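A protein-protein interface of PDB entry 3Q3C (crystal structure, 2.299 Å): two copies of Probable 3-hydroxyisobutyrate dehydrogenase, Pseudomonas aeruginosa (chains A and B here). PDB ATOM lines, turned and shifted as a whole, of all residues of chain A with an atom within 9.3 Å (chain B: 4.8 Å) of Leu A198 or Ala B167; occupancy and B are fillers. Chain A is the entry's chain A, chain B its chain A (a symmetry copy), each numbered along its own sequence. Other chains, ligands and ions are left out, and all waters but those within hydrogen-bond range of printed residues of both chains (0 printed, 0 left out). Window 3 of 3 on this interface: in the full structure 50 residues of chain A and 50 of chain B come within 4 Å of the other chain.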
ATOM      1  N   ALA A 189      -9.662  23.803 -17.684  1.00  0.00           N
ATOM      2  CA  ALA A 189     -10.599  24.046 -16.587  1.00  0.00           C
ATOM      3  C   ALA A 189     -10.917  22.724 -15.894  1.00  0.00           C
ATOM      4  O   ALA A 189     -10.796  22.616 -14.674  1.00  0.00           O
ATOM      5  CB  ALA A 189     -11.861  24.697 -17.096  1.00  0.00           C
ATOM      6  N   MET A 190     -11.293  21.719 -16.686  1.00  0.00           N
ATOM      7  CA  MET A 190     -11.421  20.358 -16.183  1.00  0.00           C
ATOM      8  C   MET A 190     -10.249  19.967 -15.264  1.00  0.00           C
ATOM      9  O   MET A 190     -10.458  19.521 -14.138  1.00  0.00           O
ATOM     10  CB  MET A 190     -11.564  19.347 -17.332  1.00  0.00           C
ATOM     11  CG  MET A 190     -12.957  19.335 -18.005  1.00  0.00           C
ATOM     12  SD  MET A 190     -14.487  19.124 -16.787  1.00  0.00           S
ATOM     13  CE  MET A 190     -14.342  17.231 -16.409  1.00  0.00           C
ATOM     14  N   ALA A 191      -9.018  20.148 -15.728  1.00  0.00           N
ATOM     15  CA  ALA A 191      -7.884  19.659 -14.965  1.00  0.00           C
ATOM     16  C   ALA A 191      -7.591  20.518 -13.730  1.00  0.00           C
ATOM     17  O   ALA A 191      -7.017  20.040 -12.744  1.00  0.00           O
ATOM     18  CB  ALA A 191      -6.642  19.524 -15.862  1.00  0.00           C
ATOM     19  N   LEU A 192      -7.995  21.779 -13.771  1.00  0.00           N
ATOM     20  CA  LEU A 192      -7.815  22.655 -12.614  1.00  0.00           C
ATOM     21  C   LEU A 192      -8.732  22.240 -11.456  1.00  0.00           C
ATOM     22  O   LEU A 192      -8.316  22.181 -10.307  1.00  0.00           O
ATOM     23  CB  LEU A 192      -8.083  24.113 -13.000  1.00  0.00           C
ATOM     24  CG  LEU A 192      -7.904  25.180 -11.908  1.00  0.00           C
ATOM     25  CD1 LEU A 192      -6.449  25.223 -11.353  1.00  0.00           C
ATOM     26  CD2 LEU A 192      -8.358  26.564 -12.412  1.00  0.00           C
ATOM     27  N   GLY A 193      -9.988  21.962 -11.770  1.00  0.00           N
ATOM     28  CA  GLY A 193     -10.941  21.580 -10.753  1.00  0.00           C
ATOM     29  C   GLY A 193     -10.577  20.237 -10.148  1.00  0.00           C
ATOM     30  O   GLY A 193     -10.518  20.086  -8.926  1.00  0.00           O
ATOM     31  N   VAL A 194     -10.331  19.255 -11.003  1.00  0.00           N
ATOM     32  CA  VAL A 194      -9.896  17.954 -10.523  1.00  0.00           C
ATOM     33  C   VAL A 194      -8.680  18.086  -9.583  1.00  0.00           C
ATOM     34  O   VAL A 194      -8.619  17.439  -8.538  1.00  0.00           O
ATOM     35  CB  VAL A 194      -9.596  16.979 -11.692  1.00  0.00           C
ATOM     36  CG1 VAL A 194      -9.124  15.622 -11.168  1.00  0.00           C
ATOM     37  CG2 VAL A 194     -10.826  16.792 -12.552  1.00  0.00           C
ATOM     38  N   ALA A 195      -7.719  18.932  -9.942  1.00  0.00           N
ATOM     39  CA  ALA A 195      -6.493  19.032  -9.153  1.00  0.00           C
ATOM     40  C   ALA A 195      -6.778  19.726  -7.822  1.00  0.00           C
ATOM     41  O   ALA A 195      -5.998  19.638  -6.876  1.00  0.00           O
ATOM     42  CB  ALA A 195      -5.428  19.775  -9.935  1.00  0.00           C
ATOM     43  N   ASN A 196      -7.906  20.420  -7.752  1.00  0.00           N
ATOM     44  CA  ASN A 196      -8.275  21.090  -6.523  1.00  0.00           C
ATOM     45  C   ASN A 196      -9.372  20.348  -5.779  1.00  0.00           C
ATOM     46  O   ASN A 196      -9.960  20.869  -4.844  1.00  0.00           O
ATOM     47  CB  ASN A 196      -8.638  22.543  -6.805  1.00  0.00           C
ATOM     48  CG  ASN A 196      -7.407  23.387  -7.111  1.00  0.00           C
ATOM     49  OD1 ASN A 196      -6.701  23.806  -6.195  1.00  0.00           O
ATOM     50  ND2 ASN A 196      -7.122  23.610  -8.405  1.00  0.00           N
ATOM     51  N   GLY A 197      -9.632  19.119  -6.212  1.00  0.00           N
ATOM     52  CA  GLY A 197     -10.371  18.170  -5.407  1.00  0.00           C
ATOM     53  C   GLY A 197     -11.736  17.785  -5.927  1.00  0.00           C
ATOM     54  O   GLY A 197     -12.430  16.978  -5.309  1.00  0.00           O
ATOM     55  N   LEU A 198     -12.130  18.348  -7.062  1.00  0.00           N
ATOM     56  CA  LEU A 198     -13.475  18.117  -7.576  1.00  0.00           C
ATOM     57  C   LEU A 198     -13.563  16.805  -8.331  1.00  0.00           C
ATOM     58  O   LEU A 198     -12.562  16.310  -8.847  1.00  0.00           O
ATOM     59  CB  LEU A 198     -13.928  19.279  -8.474  1.00  0.00           C
ATOM     60  CG  LEU A 198     -13.963  20.678  -7.826  1.00  0.00           C
ATOM     61  CD1 LEU A 198     -14.394  21.752  -8.818  1.00  0.00           C
ATOM     62  CD2 LEU A 198     -14.881  20.701  -6.621  1.00  0.00           C
ATOM     63  N   GLU A 199     -14.761  16.237  -8.381  1.00  0.00           N
ATOM     64  CA  GLU A 199     -15.009  15.069  -9.217  1.00  0.00           C
ATOM     65  C   GLU A 199     -15.275  15.557 -10.619  1.00  0.00           C
ATOM     66  O   GLU A 199     -16.102  16.454 -10.833  1.00  0.00           O
ATOM     67  CB  GLU A 199     -16.209  14.262  -8.713  1.00  0.00           C
ATOM     68  CG  GLU A 199     -15.900  13.400  -7.494  1.00  0.00           C
ATOM     69  CD  GLU A 199     -17.095  12.569  -7.026  1.00  0.00           C
ATOM     70  OE1 GLU A 199     -17.924  12.159  -7.877  1.00  0.00           O
ATOM     71  OE2 GLU A 199     -17.198  12.317  -5.803  1.00  0.00           O
ATOM     72  N   ALA A 200     -14.555  14.974 -11.566  1.00  0.00           N
ATOM     73  CA  ALA A 200     -14.613  15.384 -12.962  1.00  0.00           C
ATOM     74  C   ALA A 200     -16.053  15.550 -13.448  1.00  0.00           C
ATOM     75  O   ALA A 200     -16.412  16.584 -14.007  1.00  0.00           O
ATOM     76  CB  ALA A 200     -13.879  14.367 -13.828  1.00  0.00           C
ATOM     77  N   LYS A 201     -16.873  14.530 -13.217  1.00  0.00           N
ATOM     78  CA  LYS A 201     -18.230  14.490 -13.758  1.00  0.00           C
ATOM     79  C   LYS A 201     -19.079  15.600 -13.169  1.00  0.00           C
ATOM     80  O   LYS A 201     -19.842  16.248 -13.880  1.00  0.00           O
ATOM     81  CB  LYS A 201     -18.880  13.134 -13.480  1.00  0.00           C
ATOM     82  CG  LYS A 201     -17.974  11.959 -13.764  1.00  0.00           C
ATOM     83  CD  LYS A 201     -18.712  10.641 -13.622  1.00  0.00           C
ATOM     84  CE  LYS A 201     -19.690  10.411 -14.765  1.00  0.00           C
ATOM     85  NZ  LYS A 201     -19.276   9.252 -15.619  1.00  0.00           N
ATOM     86  N   VAL A 202     -18.940  15.805 -11.864  1.00  0.00           N
ATOM     87  CA  VAL A 202     -19.615  16.895 -11.180  1.00  0.00           C
ATOM     88  C   VAL A 202     -19.209  18.256 -11.744  1.00  0.00           C
ATOM     89  O   VAL A 202     -20.062  19.067 -12.122  1.00  0.00           O
ATOM     90  CB  VAL A 202     -19.309  16.875  -9.667  1.00  0.00           C
ATOM     91  CG1 VAL A 202     -19.901  18.104  -8.981  1.00  0.00           C
ATOM     92  CG2 VAL A 202     -19.813  15.555  -9.021  1.00  0.00           C
ATOM     93  N   LEU A 203     -17.905  18.508 -11.796  1.00  0.00           N
ATOM     94  CA  LEU A 203     -17.404  19.762 -12.348  1.00  0.00           C
ATOM     95  C   LEU A 203     -17.937  19.989 -13.752  1.00  0.00           C
ATOM     96  O   LEU A 203     -18.300  21.114 -14.112  1.00  0.00           O
ATOM     97  CB  LEU A 203     -15.885  19.773 -12.392  1.00  0.00           C
ATOM     98  CG  LEU A 203     -15.335  21.036 -13.039  1.00  0.00           C
ATOM     99  CD1 LEU A 203     -15.972  22.283 -12.428  1.00  0.00           C
ATOM    100  CD2 LEU A 203     -13.831  21.065 -12.897  1.00  0.00           C
ATOM    101  N   ALA A 204     -17.998  18.917 -14.536  1.00  0.00           N
ATOM    102  CA  ALA A 204     -18.382  19.051 -15.930  1.00  0.00           C
ATOM    103  C   ALA A 204     -19.804  19.574 -16.043  1.00  0.00           C
ATOM    104  O   ALA A 204     -20.069  20.549 -16.746  1.00  0.00           O
ATOM    105  CB  ALA A 204     -18.241  17.727 -16.653  1.00  0.00           C
ATOM    106  N   ILE A 206     -21.700  21.109 -13.934  1.00  0.00           N
ATOM    107  CA  ILE A 206     -21.810  22.468 -13.462  1.00  0.00           C
ATOM    108  C   ILE A 206     -21.466  23.464 -14.568  1.00  0.00           C
ATOM    109  O   ILE A 206     -22.251  24.361 -14.880  1.00  0.00           O
ATOM    110  CB  ILE A 206     -20.910  22.685 -12.241  1.00  0.00           C
ATOM    111  CG1 ILE A 206     -21.512  21.963 -11.026  1.00  0.00           C
ATOM    112  CG2 ILE A 206     -20.742  24.160 -11.965  1.00  0.00           C
ATOM    113  CD1 ILE A 206     -20.741  22.168  -9.725  1.00  0.00           C
ATOM    114  N   MET A 207     -20.301  23.301 -15.183  1.00  0.00           N
ATOM    115  CA  MET A 207     -19.885  24.273 -16.175  1.00  0.00           C
ATOM    116  C   MET A 207     -20.760  24.205 -17.421  1.00  0.00           C
ATOM    117  O   MET A 207     -21.024  25.236 -18.055  1.00  0.00           O
ATOM    118  CB  MET A 207     -18.409  24.109 -16.498  1.00  0.00           C
ATOM    119  CG  MET A 207     -17.526  24.348 -15.291  1.00  0.00           C
ATOM    120  SD  MET A 207     -15.656  24.483 -15.794  1.00  0.00           S
ATOM    121  CE  MET A 207     -15.784  26.131 -16.787  1.00  0.00           C
ATOM    122  N   TRP A 223     -12.311  15.071 -20.912  1.00  0.00           N
ATOM    123  CA  TRP A 223     -11.876  14.338 -19.719  1.00  0.00           C
ATOM    124  C   TRP A 223     -12.394  12.882 -19.664  1.00  0.00           C
ATOM    125  O   TRP A 223     -13.607  12.624 -19.724  1.00  0.00           O
ATOM    126  CB  TRP A 223     -12.192  15.112 -18.434  1.00  0.00           C
ATOM    127  CG  TRP A 223     -11.497  14.547 -17.219  1.00  0.00           C
ATOM    128  CD1 TRP A 223     -11.905  13.482 -16.471  1.00  0.00           C
ATOM    129  CD2 TRP A 223     -10.268  14.997 -16.634  1.00  0.00           C
ATOM    130  NE1 TRP A 223     -11.020  13.247 -15.451  1.00  0.00           N
ATOM    131  CE2 TRP A 223     -10.002  14.164 -15.525  1.00  0.00           C
ATOM    132  CE3 TRP A 223      -9.364  16.030 -16.934  1.00  0.00           C
ATOM    133  CZ2 TRP A 223      -8.866  14.321 -14.708  1.00  0.00           C
ATOM    134  CZ3 TRP A 223      -8.238  16.188 -16.124  1.00  0.00           C
ATOM    135  CH2 TRP A 223      -7.998  15.332 -15.021  1.00  0.00           C
ATOM    136  N   ASP B 119     -19.673  27.266   1.714  1.00  0.00           N
ATOM    137  CA  ASP B 119     -19.299  28.252   0.697  1.00  0.00           C
ATOM    138  C   ASP B 119     -20.274  28.094  -0.464  1.00  0.00           C
ATOM    139  O   ASP B 119     -20.413  27.008  -1.035  1.00  0.00           O
ATOM    140  CB  ASP B 119     -17.820  28.166   0.275  1.00  0.00           C
ATOM    141  CG  ASP B 119     -17.426  26.809  -0.298  1.00  0.00           C
ATOM    142  OD1 ASP B 119     -17.699  25.763   0.333  1.00  0.00           O
ATOM    143  OD2 ASP B 119     -16.807  26.797  -1.383  1.00  0.00           O
ATOM    144  N   VAL B 138     -21.916  24.986  -4.359  1.00  0.00           N
ATOM    145  CA  VAL B 138     -21.804  24.821  -2.914  1.00  0.00           C
ATOM    146  C   VAL B 138     -20.768  23.777  -2.501  1.00  0.00           C
ATOM    147  O   VAL B 138     -20.799  22.651  -2.982  1.00  0.00           O
ATOM    148  CB  VAL B 138     -23.180  24.395  -2.343  1.00  0.00           C
ATOM    149  CG1 VAL B 138     -23.202  24.454  -0.810  1.00  0.00           C
ATOM    150  CG2 VAL B 138     -24.273  25.262  -2.936  1.00  0.00           C
ATOM    151  N   GLY B 139     -19.850  24.163  -1.618  1.00  0.00           N
ATOM    152  CA  GLY B 139     -19.018  23.214  -0.895  1.00  0.00           C
ATOM    153  C   GLY B 139     -19.630  22.976   0.483  1.00  0.00           C
ATOM    154  O   GLY B 139     -20.428  23.800   0.930  1.00  0.00           O
ATOM    155  N   ALA B 162     -21.205  20.991  -5.132  1.00  0.00           N
ATOM    156  CA  ALA B 162     -19.936  20.819  -5.832  1.00  0.00           C
ATOM    157  C   ALA B 162     -18.903  19.987  -5.064  1.00  0.00           C
ATOM    158  O   ALA B 162     -17.932  19.530  -5.645  1.00  0.00           O
ATOM    159  CB  ALA B 162     -19.358  22.169  -6.213  1.00  0.00           C
ATOM    160  N   GLY B 163     -19.110  19.792  -3.764  1.00  0.00           N
ATOM    161  CA  GLY B 163     -18.201  18.977  -2.978  1.00  0.00           C
ATOM    162  C   GLY B 163     -18.152  19.439  -1.539  1.00  0.00           C
ATOM    163  O   GLY B 163     -19.115  20.020  -1.043  1.00  0.00           O
ATOM    164  N   PRO B 164     -17.030  19.171  -0.854  1.00  0.00           N
ATOM    165  CA  PRO B 164     -16.841  19.569   0.551  1.00  0.00           C
ATOM    166  C   PRO B 164     -16.243  20.961   0.679  1.00  0.00           C
ATOM    167  O   PRO B 164     -16.105  21.663  -0.327  1.00  0.00           O
ATOM    168  CB  PRO B 164     -15.867  18.513   1.084  1.00  0.00           C
ATOM    169  CG  PRO B 164     -15.087  18.063  -0.137  1.00  0.00           C
ATOM    170  CD  PRO B 164     -15.957  18.290  -1.346  1.00  0.00           C
ATOM    171  N   ASP B 165     -15.899  21.350   1.904  1.00  0.00           N
ATOM    172  CA  ASP B 165     -15.372  22.684   2.176  1.00  0.00           C
ATOM    173  C   ASP B 165     -14.535  23.198   1.003  1.00  0.00           C
ATOM    174  O   ASP B 165     -13.499  22.624   0.674  1.00  0.00           O
ATOM    175  CB  ASP B 165     -14.521  22.686   3.455  1.00  0.00           C
ATOM    176  CG  ASP B 165     -15.320  22.321   4.704  1.00  0.00           C
ATOM    177  OD1 ASP B 165     -16.486  21.882   4.568  1.00  0.00           O
ATOM    178  OD2 ASP B 165     -14.775  22.478   5.825  1.00  0.00           O
ATOM    179  N   GLY B 166     -14.995  24.269   0.368  1.00  0.00           N
ATOM    180  CA  GLY B 166     -14.184  24.940  -0.621  1.00  0.00           C
ATOM    181  C   GLY B 166     -14.568  24.628  -2.050  1.00  0.00           C
ATOM    182  O   GLY B 166     -14.274  25.411  -2.950  1.00  0.00           O
ATOM    183  N   ALA B 167     -15.237  23.498  -2.254  1.00  0.00           N
ATOM    184  CA  ALA B 167     -15.591  23.050  -3.599  1.00  0.00           C
ATOM    185  C   ALA B 167     -16.400  24.093  -4.372  1.00  0.00           C
ATOM    186  O   ALA B 167     -16.276  24.208  -5.603  1.00  0.00           O
ATOM    187  CB  ALA B 167     -16.354  21.742  -3.542  1.00  0.00           C
ATOM    188  N   GLY B 168     -17.241  24.834  -3.654  1.00  0.00           N
ATOM    189  CA  GLY B 168     -18.048  25.844  -4.295  1.00  0.00           C
ATOM    190  C   GLY B 168     -17.150  26.825  -5.022  1.00  0.00           C
ATOM    191  O   GLY B 168     -17.265  27.007  -6.227  1.00  0.00           O
ATOM    192  N   GLN B 169     -16.245  27.443  -4.271  1.00  0.00           N
ATOM    193  CA  GLN B 169     -15.315  28.409  -4.818  1.00  0.00           C
ATOM    194  C   GLN B 169     -14.528  27.805  -5.965  1.00  0.00           C
ATOM    195  O   GLN B 169     -14.222  28.499  -6.929  1.00  0.00           O
ATOM    196  CB  GLN B 169     -14.343  28.906  -3.749  1.00  0.00           C
ATOM    197  CG  GLN B 169     -15.001  29.506  -2.528  1.00  0.00           C
ATOM    198  CD  GLN B 169     -15.857  30.722  -2.842  1.00  0.00           C
ATOM    199  OE1 GLN B 169     -15.944  31.169  -3.997  1.00  0.00           O
ATOM    200  NE2 GLN B 169     -16.496  31.267  -1.811  1.00  0.00           N
ATOM    201  N   VAL B 170     -14.207  26.517  -5.872  1.00  0.00           N
ATOM    202  CA  VAL B 170     -13.362  25.899  -6.890  1.00  0.00           C
ATOM    203  C   VAL B 170     -14.133  25.847  -8.201  1.00  0.00           C
ATOM    204  O   VAL B 170     -13.614  26.171  -9.266  1.00  0.00           O
ATOM    205  CB  VAL B 170     -12.902  24.466  -6.500  1.00  0.00           C
ATOM    206  CG1 VAL B 170     -12.071  23.848  -7.615  1.00  0.00           C
ATOM    207  CG2 VAL B 170     -12.129  24.459  -5.179  1.00  0.00           C
ATOM    208  N   ALA B 171     -15.387  25.435  -8.112  1.00  0.00           N
ATOM    209  CA  ALA B 171     -16.199  25.259  -9.304  1.00  0.00           C
ATOM    210  C   ALA B 171     -16.459  26.614  -9.938  1.00  0.00           C
ATOM    211  O   ALA B 171     -16.446  26.746 -11.155  1.00  0.00           O
ATOM    212  CB  ALA B 171     -17.512  24.566  -8.950  1.00  0.00           C
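N of Ala B162 is in hydrogen-bond range of O of Val B138 (2.7 Å). The backbone carbonyl oxygen (O) of Leu A192 sits at hydrogen-bond distance from the side-chain amide nitrogen (ND2) of Asn A196 (2.7 Å). The backbone NH of Leu A198 is in hydrogen-bond range of the backbone carbonyl oxygen of Gly A193, at 3.0 Å.
Among the printed residues, merely in contact across the chains: Asn A196 with Val B170 (3.8 Å), Leu A198 with Ala B162 (3.4 Å), Leu A198 with Ala B167 (3.6 Å), Leu A198 with Val B170 (3.4 Å), Leu A198 with Ala B171 (3.9 Å) and Ile A206 with Ala B162 (3.8 Å).
Of the printed residues of chain B, Asn A196 touches Val B170 (3.8 Å). Of the printed residues of chain B, Ile A206 touches Ala B162. Of chain A, only Leu A198 (3.4 Å) and Ile A206 (3.8 Å) come within 4 Å of Ala B162. Gly B163 touches none of the printed residues of chain A. No residue of chain A comes within 4 Å of Gly B166. Ala B167 touches just one residue of chain A: Leu A198 (3.6 Å). Of chain A, only Asn A196 (3.8 Å) and Leu A198 (3.4 Å) come within 4 Å of Val B170. Printed residues of chain A within 4 Å of Ala B171: Leu A198 (3.9 Å). The nearest printed residue of chain B that does not touch Leu A198 is Gly B163 (5.2 Å). The nearest residue of chain A that does not touch Ala B167 is Asn A196 (6.2 Å).
Of the 19 printed residues of chain A, 3 touch a printed residue of chain B. Hydrophobic or aromatic side chains of chain B that line the printed part of chain A: Ala B162, Ala B167 and Val B170. Among the printed residues, 6 pairs touch across the chains. Among the printed residues, no Asp or Glu carboxylate lies within 4 Å of a Lys or Arg side-chain nitrogen of the other chain.
No position is printed for both chains. Of the 6 pairs that touch across the chains among the printed residues, none has its exchanged pair printed and touching as well.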
